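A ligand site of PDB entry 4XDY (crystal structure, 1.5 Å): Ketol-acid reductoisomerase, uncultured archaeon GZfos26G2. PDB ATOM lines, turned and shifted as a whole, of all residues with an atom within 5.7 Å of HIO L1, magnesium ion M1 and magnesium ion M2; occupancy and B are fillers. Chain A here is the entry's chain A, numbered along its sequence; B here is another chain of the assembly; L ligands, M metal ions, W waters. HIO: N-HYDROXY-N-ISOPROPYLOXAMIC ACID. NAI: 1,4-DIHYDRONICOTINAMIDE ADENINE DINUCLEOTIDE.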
ATOM      1  N   ASP A  87       1.172  -4.715 -16.800  1.00  0.00           N
ATOM      2  CA  ASP A  87       1.469  -3.752 -15.725  1.00  0.00           C
ATOM      3  C   ASP A  87       1.005  -4.234 -14.362  1.00  0.00           C
ATOM      4  O   ASP A  87       1.693  -4.057 -13.356  1.00  0.00           O
ATOM      5  CB  ASP A  87       0.911  -2.352 -15.974  1.00  0.00           C
ATOM      6  CG  ASP A  87       1.419  -1.773 -17.289  1.00  0.00           C
ATOM      7  OD1 ASP A  87       2.661  -1.467 -17.348  1.00  0.00           O
ATOM      8  OD2 ASP A  87       0.635  -1.711 -18.270  1.00  0.00           O
ATOM      9  N   HIS A 112       6.416   1.195 -20.312  1.00  0.00           N
ATOM     10  CA  HIS A 112       5.374   2.107 -19.856  1.00  0.00           C
ATOM     11  C   HIS A 112       5.825   2.500 -18.466  1.00  0.00           C
ATOM     12  O   HIS A 112       6.242   1.596 -17.669  1.00  0.00           O
ATOM     13  CB  HIS A 112       4.046   1.362 -19.772  1.00  0.00           C
ATOM     14  CG  HIS A 112       2.878   2.185 -19.340  1.00  0.00           C
ATOM     15  ND1 HIS A 112       2.704   3.548 -19.650  1.00  0.00           N
ATOM     16  CD2 HIS A 112       1.789   1.822 -18.614  1.00  0.00           C
ATOM     17  CE1 HIS A 112       1.516   3.932 -19.176  1.00  0.00           C
ATOM     18  NE2 HIS A 112       0.947   2.900 -18.552  1.00  0.00           N
ATOM     19  N   PRO A 134       7.126   2.432 -26.850  1.00  0.00           N
ATOM     20  CA  PRO A 134       6.720   2.637 -28.223  1.00  0.00           C
ATOM     21  C   PRO A 134       5.300   3.192 -28.214  1.00  0.00           C
ATOM     22  O   PRO A 134       4.483   2.672 -27.473  1.00  0.00           O
ATOM     23  CB  PRO A 134       6.770   1.207 -28.840  1.00  0.00           C
ATOM     24  CG  PRO A 134       6.524   0.318 -27.666  1.00  0.00           C
ATOM     25  CD  PRO A 134       6.945   1.028 -26.430  1.00  0.00           C
ATOM     26  N   LYS A 135       5.003   4.128 -29.114  1.00  0.00           N
ATOM     27  CA  LYS A 135       3.675   4.700 -29.291  1.00  0.00           C
ATOM     28  C   LYS A 135       2.984   3.858 -30.376  1.00  0.00           C
ATOM     29  O   LYS A 135       2.738   4.284 -31.540  1.00  0.00           O
ATOM     30  CB  LYS A 135       3.785   6.210 -29.667  1.00  0.00           C
ATOM     31  CG  LYS A 135       4.519   7.049 -28.654  1.00  0.00           C
ATOM     32  CD  LYS A 135       3.828   7.181 -27.308  1.00  0.00           C
ATOM     33  CE  LYS A 135       4.253   6.200 -26.209  1.00  0.00           C
ATOM     34  NZ  LYS A 135       3.517   6.272 -24.863  1.00  0.00           N
ATOM     35  N   ALA A 136       2.757   2.554 -30.041  1.00  0.00           N
ATOM     36  CA  ALA A 136       2.300   1.598 -30.999  1.00  0.00           C
ATOM     37  C   ALA A 136       1.889   0.292 -30.327  1.00  0.00           C
ATOM     38  O   ALA A 136       2.547  -0.168 -29.387  1.00  0.00           O
ATOM     39  CB  ALA A 136       3.354   1.271 -32.000  1.00  0.00           C
ATOM     40  N   PRO A 137       0.794  -0.308 -30.830  1.00  0.00           N
ATOM     41  CA  PRO A 137       0.553  -1.690 -30.473  1.00  0.00           C
ATOM     42  C   PRO A 137       1.663  -2.651 -31.030  1.00  0.00           C
ATOM     43  O   PRO A 137       2.181  -2.468 -32.129  1.00  0.00           O
ATOM     44  CB  PRO A 137      -0.817  -2.002 -31.085  1.00  0.00           C
ATOM     45  CG  PRO A 137      -0.888  -1.076 -32.248  1.00  0.00           C
ATOM     46  CD  PRO A 137      -0.114   0.154 -31.869  1.00  0.00           C
ATOM     47  N   GLY A 138       1.941  -3.705 -30.296  1.00  0.00           N
ATOM     48  CA  GLY A 138       3.130  -4.476 -30.588  1.00  0.00           C
ATOM     49  C   GLY A 138       3.131  -5.163 -31.959  1.00  0.00           C
ATOM     50  O   GLY A 138       4.174  -5.260 -32.603  1.00  0.00           O
ATOM     51  N   GLU A 191       5.506  10.225 -19.787  1.00  0.00           N
ATOM     52  CA  GLU A 191       5.042   9.082 -20.563  1.00  0.00           C
ATOM     53  C   GLU A 191       3.820   8.452 -19.964  1.00  0.00           C
ATOM     54  O   GLU A 191       2.842   8.230 -20.682  1.00  0.00           O
ATOM     55  CB  GLU A 191       6.097   8.008 -20.720  1.00  0.00           C
ATOM     56  CG  GLU A 191       5.698   6.991 -21.803  1.00  0.00           C
ATOM     57  CD  GLU A 191       4.790   5.821 -21.350  1.00  0.00           C
ATOM     58  OE1 GLU A 191       4.704   5.550 -20.145  1.00  0.00           O
ATOM     59  OE2 GLU A 191       4.221   5.252 -22.289  1.00  0.00           O
ATOM     60  N   ASP A 195       0.282   8.647 -22.005  1.00  0.00           N
ATOM     61  CA  ASP A 195      -0.056   7.291 -22.543  1.00  0.00           C
ATOM     62  C   ASP A 195      -1.436   6.858 -22.052  1.00  0.00           C
ATOM     63  O   ASP A 195      -2.257   6.429 -22.842  1.00  0.00           O
ATOM     64  CB  ASP A 195       0.995   6.284 -22.103  1.00  0.00           C
ATOM     65  CG  ASP A 195       0.782   4.938 -22.773  1.00  0.00           C
ATOM     66  OD1 ASP A 195       1.117   4.826 -23.968  1.00  0.00           O
ATOM     67  OD2 ASP A 195       0.189   4.067 -22.091  1.00  0.00           O
ATOM     68  N   LEU A 196      -1.630   6.958 -20.774  1.00  0.00           N
ATOM     69  CA  LEU A 196      -2.917   6.637 -20.146  1.00  0.00           C
ATOM     70  C   LEU A 196      -4.021   7.501 -20.734  1.00  0.00           C
ATOM     71  O   LEU A 196      -5.050   6.993 -21.171  1.00  0.00           O
ATOM     72  CB  LEU A 196      -2.830   6.788 -18.674  1.00  0.00           C
ATOM     73  CG  LEU A 196      -2.015   5.750 -17.894  1.00  0.00           C
ATOM     74  CD1 LEU A 196      -2.020   6.117 -16.426  1.00  0.00           C
ATOM     75  CD2 LEU A 196      -2.553   4.323 -18.002  1.00  0.00           C
ATOM     76  N   GLU A 199      -4.762   6.444 -24.590  1.00  0.00           N
ATOM     77  CA  GLU A 199      -5.459   5.209 -24.822  1.00  0.00           C
ATOM     78  C   GLU A 199      -6.931   5.361 -24.315  1.00  0.00           C
ATOM     79  O   GLU A 199      -7.836   4.800 -24.953  1.00  0.00           O
ATOM     80  CB  GLU A 199      -4.726   4.007 -24.181  1.00  0.00           C
ATOM     81  CG  GLU A 199      -4.616   4.021 -22.706  1.00  0.00           C
ATOM     82  CD  GLU A 199      -3.423   3.257 -22.125  1.00  0.00           C
ATOM     83  OE1 GLU A 199      -2.409   2.991 -22.861  1.00  0.00           O
ATOM     84  OE2 GLU A 199      -3.523   2.856 -20.935  1.00  0.00           O
ATOM     85  N   LEU A 203      -7.361   6.943 -28.524  1.00  0.00           N
ATOM     86  CA  LEU A 203      -7.046   5.791 -29.330  1.00  0.00           C
ATOM     87  C   LEU A 203      -7.955   4.567 -29.122  1.00  0.00           C
ATOM     88  O   LEU A 203      -8.249   3.859 -30.107  1.00  0.00           O
ATOM     89  CB  LEU A 203      -5.613   5.346 -29.071  1.00  0.00           C
ATOM     90  CG  LEU A 203      -4.444   6.305 -29.355  1.00  0.00           C
ATOM     91  CD1 LEU A 203      -3.126   5.706 -28.866  1.00  0.00           C
ATOM     92  CD2 LEU A 203      -4.374   6.587 -30.843  1.00  0.00           C
ATOM     93  N   CYS A 204      -8.359   4.300 -27.900  1.00  0.00           N
ATOM     94  CA  CYS A 204      -9.092   3.054 -27.622  1.00  0.00           C
ATOM     95  C   CYS A 204     -10.494   3.475 -27.085  1.00  0.00           C
ATOM     96  O   CYS A 204     -11.481   3.202 -27.729  1.00  0.00           O
ATOM     97  CB  CYS A 204      -8.346   2.179 -26.634  1.00  0.00           C
ATOM     98  SG  CYS A 204      -6.661   1.767 -27.190  1.00  0.00           S
ATOM     99  N   GLU B 231       0.842  10.390 -30.038  1.00  0.00           N
ATOM    100  CA  GLU B 231      -0.158   9.716 -29.225  1.00  0.00           C
ATOM    101  C   GLU B 231      -1.539   9.759 -29.872  1.00  0.00           C
ATOM    102  O   GLU B 231      -2.257   8.731 -29.842  1.00  0.00           O
ATOM    103  CB  GLU B 231      -0.175  10.301 -27.825  1.00  0.00           C
ATOM    104  CG  GLU B 231      -1.138   9.666 -26.833  1.00  0.00           C
ATOM    105  CD  GLU B 231      -0.755   8.241 -26.460  1.00  0.00           C
ATOM    106  OE1 GLU B 231       0.481   8.027 -26.200  1.00  0.00           O
ATOM    107  OE2 GLU B 231      -1.662   7.386 -26.232  1.00  0.00           O
ATOM    108  N   GLU B 235      -0.513   7.186 -33.913  1.00  0.00           N
ATOM    109  CA  GLU B 235      -0.854   5.872 -33.410  1.00  0.00           C
ATOM    110  C   GLU B 235      -2.313   5.476 -33.782  1.00  0.00           C
ATOM    111  O   GLU B 235      -2.586   4.266 -33.794  1.00  0.00           O
ATOM    112  CB  GLU B 235      -0.650   5.804 -31.886  1.00  0.00           C
ATOM    113  CG  GLU B 235      -0.718   4.370 -31.388  1.00  0.00           C
ATOM    114  CD  GLU B 235      -0.238   4.160 -29.977  1.00  0.00           C
ATOM    115  OE1 GLU B 235       0.283   5.093 -29.349  1.00  0.00           O
ATOM    116  OE2 GLU B 235      -0.452   3.005 -29.474  1.00  0.00           O
ATOM    117  N   ILE B 239      -3.883   1.480 -34.379  1.00  0.00           N
ATOM    118  CA  ILE B 239      -4.990   0.908 -33.610  1.00  0.00           C
ATOM    119  C   ILE B 239      -6.158   0.611 -34.528  1.00  0.00           C
ATOM    120  O   ILE B 239      -6.747  -0.523 -34.450  1.00  0.00           O
ATOM    121  CB  ILE B 239      -5.414   1.860 -32.485  1.00  0.00           C
ATOM    122  CG1 ILE B 239      -4.258   2.080 -31.515  1.00  0.00           C
ATOM    123  CG2 ILE B 239      -6.684   1.389 -31.851  1.00  0.00           C
ATOM    124  CD1 ILE B 239      -3.776   0.809 -30.868  1.00  0.00           C
ATOM    125  N   VAL B 254      -4.612  -7.091 -28.265  1.00  0.00           N
ATOM    126  CA  VAL B 254      -3.214  -6.680 -28.542  1.00  0.00           C
ATOM    127  C   VAL B 254      -2.787  -5.561 -27.600  1.00  0.00           C
ATOM    128  O   VAL B 254      -1.673  -5.553 -27.111  1.00  0.00           O
ATOM    129  CB  VAL B 254      -3.051  -6.231 -30.018  1.00  0.00           C
ATOM    130  CG1 VAL B 254      -1.698  -5.626 -30.234  1.00  0.00           C
ATOM    131  CG2 VAL B 254      -3.274  -7.416 -30.956  1.00  0.00           C
ATOM    132  N   ILE B 255      -3.693  -4.655 -27.296  1.00  0.00           N
ATOM    133  CA  ILE B 255      -3.362  -3.541 -26.387  1.00  0.00           C
ATOM    134  C   ILE B 255      -3.180  -4.129 -24.977  1.00  0.00           C
ATOM    135  O   ILE B 255      -3.590  -5.278 -24.702  1.00  0.00           O
ATOM    136  CB  ILE B 255      -4.446  -2.447 -26.332  1.00  0.00           C
ATOM    137  CG1 ILE B 255      -5.733  -2.958 -25.627  1.00  0.00           C
ATOM    138  CG2 ILE B 255      -4.658  -1.844 -27.683  1.00  0.00           C
ATOM    139  CD1 ILE B 255      -6.827  -1.923 -25.582  1.00  0.00           C
ATOM    140  N   SER B 256      -2.568  -3.363 -24.116  1.00  0.00           N
ATOM    141  CA  SER B 256      -2.365  -3.852 -22.760  1.00  0.00           C
ATOM    142  C   SER B 256      -3.637  -4.031 -22.018  1.00  0.00           C
ATOM    143  O   SER B 256      -4.623  -3.365 -22.304  1.00  0.00           O
ATOM    144  CB  SER B 256      -1.435  -2.948 -21.978  1.00  0.00           C
ATOM    145  OG  SER B 256      -2.027  -1.718 -21.631  1.00  0.00           O
ATOM    146  N   THR B 258      -3.986  -2.773 -19.124  1.00  0.00           N
ATOM    147  CA  THR B 258      -4.156  -1.451 -18.611  1.00  0.00           C
ATOM    148  C   THR B 258      -5.018  -0.585 -19.542  1.00  0.00           C
ATOM    149  O   THR B 258      -5.948   0.090 -19.082  1.00  0.00           O
ATOM    150  CB  THR B 258      -2.777  -0.766 -18.392  1.00  0.00           C
ATOM    151  OG1 THR B 258      -2.003  -1.599 -17.519  1.00  0.00           O
ATOM    152  CG2 THR B 258      -2.890   0.608 -17.816  1.00  0.00           C
ATOM    153  N   ALA B 259      -4.660  -0.618 -20.834  1.00  0.00           N
ATOM    154  CA  ALA B 259      -5.364   0.151 -21.863  1.00  0.00           C
ATOM    155  C   ALA B 259      -6.777  -0.362 -22.059  1.00  0.00           C
ATOM    156  O   ALA B 259      -7.694   0.423 -22.337  1.00  0.00           O
ATOM    157  CB  ALA B 259      -4.639   0.031 -23.149  1.00  0.00           C
HETATM  158  C1  HIO L   1      -1.219   0.143 -24.335  1.00  0.00           C
HETATM  159  O11 HIO L   1      -1.192   0.331 -23.084  1.00  0.00           O
HETATM  160  O12 HIO L   1      -1.491  -0.926 -24.977  1.00  0.00           O
HETATM  161  C2  HIO L   1      -0.758   1.402 -25.069  1.00  0.00           C
HETATM  162  O2  HIO L   1      -0.144   2.275 -24.398  1.00  0.00           O
HETATM  163  N3  HIO L   1      -1.081   1.672 -26.325  1.00  0.00           N
HETATM  164  O3  HIO L   1      -0.330   2.690 -27.048  1.00  0.00           O
HETATM  165  C4  HIO L   1      -2.092   0.964 -27.051  1.00  0.00           C
HETATM  166  C41 HIO L   1      -3.025   1.994 -27.706  1.00  0.00           C
HETATM  167  C42 HIO L   1      -1.357   0.081 -28.045  1.00  0.00           C
HETATM  168  PA  NAI L   2       0.926  -9.016 -22.202  1.00  0.00           P
HETATM  169  O1A NAI L   2      -0.429  -8.796 -21.521  1.00  0.00           O
HETATM  170  O2A NAI L   2       0.985  -9.347 -23.627  1.00  0.00           O
HETATM  171  O5B NAI L   2       1.746 -10.000 -21.215  1.00  0.00           O
HETATM  172  C5B NAI L   2       3.050 -10.507 -21.615  1.00  0.00           C
HETATM  173  C4B NAI L   2       3.128 -12.011 -21.192  1.00  0.00           C
HETATM  174  O4B NAI L   2       3.135 -11.997 -19.769  1.00  0.00           O
HETATM  175  C3B NAI L   2       1.960 -12.952 -21.583  1.00  0.00           C
HETATM  176  O3B NAI L   2       2.115 -13.291 -22.965  1.00  0.00           O
HETATM  177  C2B NAI L   2       2.129 -14.086 -20.585  1.00  0.00           C
HETATM  178  O2B NAI L   2       3.018 -15.052 -21.149  1.00  0.00           O
HETATM  179  C1B NAI L   2       2.776 -13.347 -19.387  1.00  0.00           C
HETATM  180  N9A NAI L   2       1.865 -13.273 -18.264  1.00  0.00           N
HETATM  181  C8A NAI L   2       0.528 -12.874 -18.381  1.00  0.00           C
HETATM  182  N7A NAI L   2      -0.040 -12.906 -17.181  1.00  0.00           N
HETATM  183  C5A NAI L   2       0.904 -13.362 -16.313  1.00  0.00           C
HETATM  184  C6A NAI L   2       0.927 -13.670 -14.898  1.00  0.00           C
HETATM  185  N6A NAI L   2      -0.153 -13.525 -14.126  1.00  0.00           N
HETATM  186  N1A NAI L   2       2.090 -14.078 -14.313  1.00  0.00           N
HETATM  187  C2A NAI L   2       3.199 -14.265 -15.055  1.00  0.00           C
HETATM  188  N3A NAI L   2       3.276 -14.018 -16.355  1.00  0.00           N
HETATM  189  C4A NAI L   2       2.157 -13.576 -17.030  1.00  0.00           C
HETATM  190  O3  NAI L   2       1.811  -7.593 -21.937  1.00  0.00           O
HETATM  191  PN  NAI L   2       1.823  -6.328 -23.028  1.00  0.00           P
HETATM  192  O1N NAI L   2       0.406  -5.908 -23.347  1.00  0.00           O
HETATM  193  O2N NAI L   2       2.717  -6.747 -24.111  1.00  0.00           O
HETATM  194  O5D NAI L   2       2.361  -5.239 -22.007  1.00  0.00           O
HETATM  195  C5D NAI L   2       3.782  -5.251 -21.657  1.00  0.00           C
HETATM  196  C4D NAI L   2       4.251  -3.830 -21.191  1.00  0.00           C
HETATM  197  O4D NAI L   2       4.248  -3.058 -22.412  1.00  0.00           O
HETATM  198  C3D NAI L   2       3.321  -3.085 -20.253  1.00  0.00           C
HETATM  199  O3D NAI L   2       4.081  -2.256 -19.355  1.00  0.00           O
HETATM  200  C2D NAI L   2       2.441  -2.196 -21.153  1.00  0.00           C
HETATM  201  O2D NAI L   2       1.839  -1.054 -20.537  1.00  0.00           O
HETATM  202  C1D NAI L   2       3.443  -1.831 -22.228  1.00  0.00           C
HETATM  203  N1N NAI L   2       2.962  -1.447 -23.557  1.00  0.00           N
HETATM  204  C2N NAI L   2       2.150  -2.299 -24.222  1.00  0.00           C
HETATM  205  C3N NAI L   2       1.701  -2.005 -25.462  1.00  0.00           C
HETATM  206  C7N NAI L   2       0.937  -2.971 -26.179  1.00  0.00           C
HETATM  207  O7N NAI L   2       0.267  -3.935 -25.697  1.00  0.00           O
HETATM  208  N7N NAI L   2       1.163  -2.954 -27.469  1.00  0.00           N
HETATM  209  C4N NAI L   2       2.123  -0.750 -26.069  1.00  0.00           C
HETATM  210  C5N NAI L   2       3.145  -0.017 -25.396  1.00  0.00           C
HETATM  211  C6N NAI L   2       3.507  -0.383 -24.141  1.00  0.00           C
HETATM  212 MG    MG M   1      -0.567   2.190 -22.471  1.00  0.00          MG
HETATM  213 MG    MG M   2       0.378   3.843 -25.563  1.00  0.00          MG
HETATM  214  O   HOH W   1      -1.444   4.857 -25.220  1.00  0.00           O
HETATM  215  O   HOH W   2       0.989   5.480 -26.877  1.00  0.00           O
HETATM  216  O   HOH W   3      -1.186   1.909 -20.506  1.00  0.00           O
HETATM  217  O   HOH W   4       2.457   3.142 -25.604  1.00  0.00           O
HETATM  218  O   HOH W   5       1.380   1.385 -22.016  1.00  0.00           O
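OG of Ser 256 of chain B sits close to O12 of HIO L1 (3.5 Å).
The side-chain carboxylate (OD1) of Asp 87 sits at hydrogen-bond distance from an oxygen (O3D) of NAI L2.
The side-chain carboxylate (OE2) of Glu 235 of chain B lies close to an oxygen (O3) of HIO L1 (2.4 Å).
The backbone NH of Ser 256 of chain B sits at hydrogen-bond distance from an oxygen (O12) of HIO L1 (2.8 Å).
The backbone NH (N) of Ser 256 of chain B sits at hydrogen-bond distance from an oxygen (O7N) of NAI L2 (3.3 Å).
OE2 of Glu 235 of chain B is in hydrogen-bond range of N of Ala 136 (3.3 Å).
N of Thr 258 of chain B sits close to OG of Ser 256 of chain B (3.4 Å).
The backbone NH of Cys 204 is in hydrogen-bond range of the backbone carbonyl oxygen of Glu 199, at 3.0 Å.
The side-chain hydroxyl of Ser 256 of chain B is in hydrogen-bond range of the backbone NH of Ala 259 of chain B (3.0 Å).
NZ of Lys 135 lies close to OD1 of Asp 195.
Merely in contact with HIO L1: Ala 136, Pro 137, Leu 203, Cys 204, Ile 239 of chain B, Ile 255 of chain B and Ala 259 of chain B.
Hydrophobic or aromatic side chains that line HIO L1: Pro 137, Leu 203, Ile 239 of chain B, Ile 255 of chain B and Ala 259 of chain B.
Of the 21 residues printed, 11 come within 4 Å of HIO L1.
The nearest printed residue that does not touch HIO L1 is Pro 134 (4.8 Å).
Of the 21 residues printed, 2 come within 4 Å of magnesium ion M1.
Along chain A the residues within 4 Å of magnesium ion M1 span positions 195 to 199.
The nearest printed residue that does not touch magnesium ion M1 is Ser 256 of chain B (4.3 Å).
Glu 235 of chain B touches magnesium ion M2.
Of the 21 residues printed, 3 come within 4 Å of magnesium ion M2.
Along chain A the residues within 4 Å of magnesium ion M2 span positions 195 to 199.
Magnesium ion M1 is bound by O2 of HIO L1 (2.0 Å), OE1 of Glu 199 (2.0 Å), O11 of HIO L1 (2.1 Å), OD2 of Asp 195 (2.1 Å), water W3 (2.1 Å) and water W5 (2.2 Å).
Magnesium ion M2 is bound by O3 of HIO L1 (2.0 Å), OD1 of Asp 195 (2.0 Å), O2 of HIO L1 (2.0 Å), water W1 (2.1 Å), water W2 (2.2 Å) and water W4 (2.2 Å).
Magnesium ion M2 has six donor atoms within binding distance.
Water W3 lies within hydrogen-bond range of OE2 of Glu 199 and NE2 of His 112.
Water W5 bridges an oxygen (O2D) of NAI L2 and a ring nitrogen (ND1) of His 112.
Water W1 lies within hydrogen-bond range of OE2 of Glu 231 of chain B and O of Asp 195.
Water W2 lies within hydrogen-bond range of the side-chain carboxylate (OE1) of Glu 235 of chain B (2.6 Å), the side-chain carboxylate (OE1) of Glu 231 of chain B (2.7 Å) and the side-chain amino group (NZ) of Lys 135 (3.3 Å).
Water W4 lies within hydrogen-bond range of the backbone carbonyl oxygen of Pro 134 (2.8 Å) and the side-chain amino group of Lys 135 (3.4 Å).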
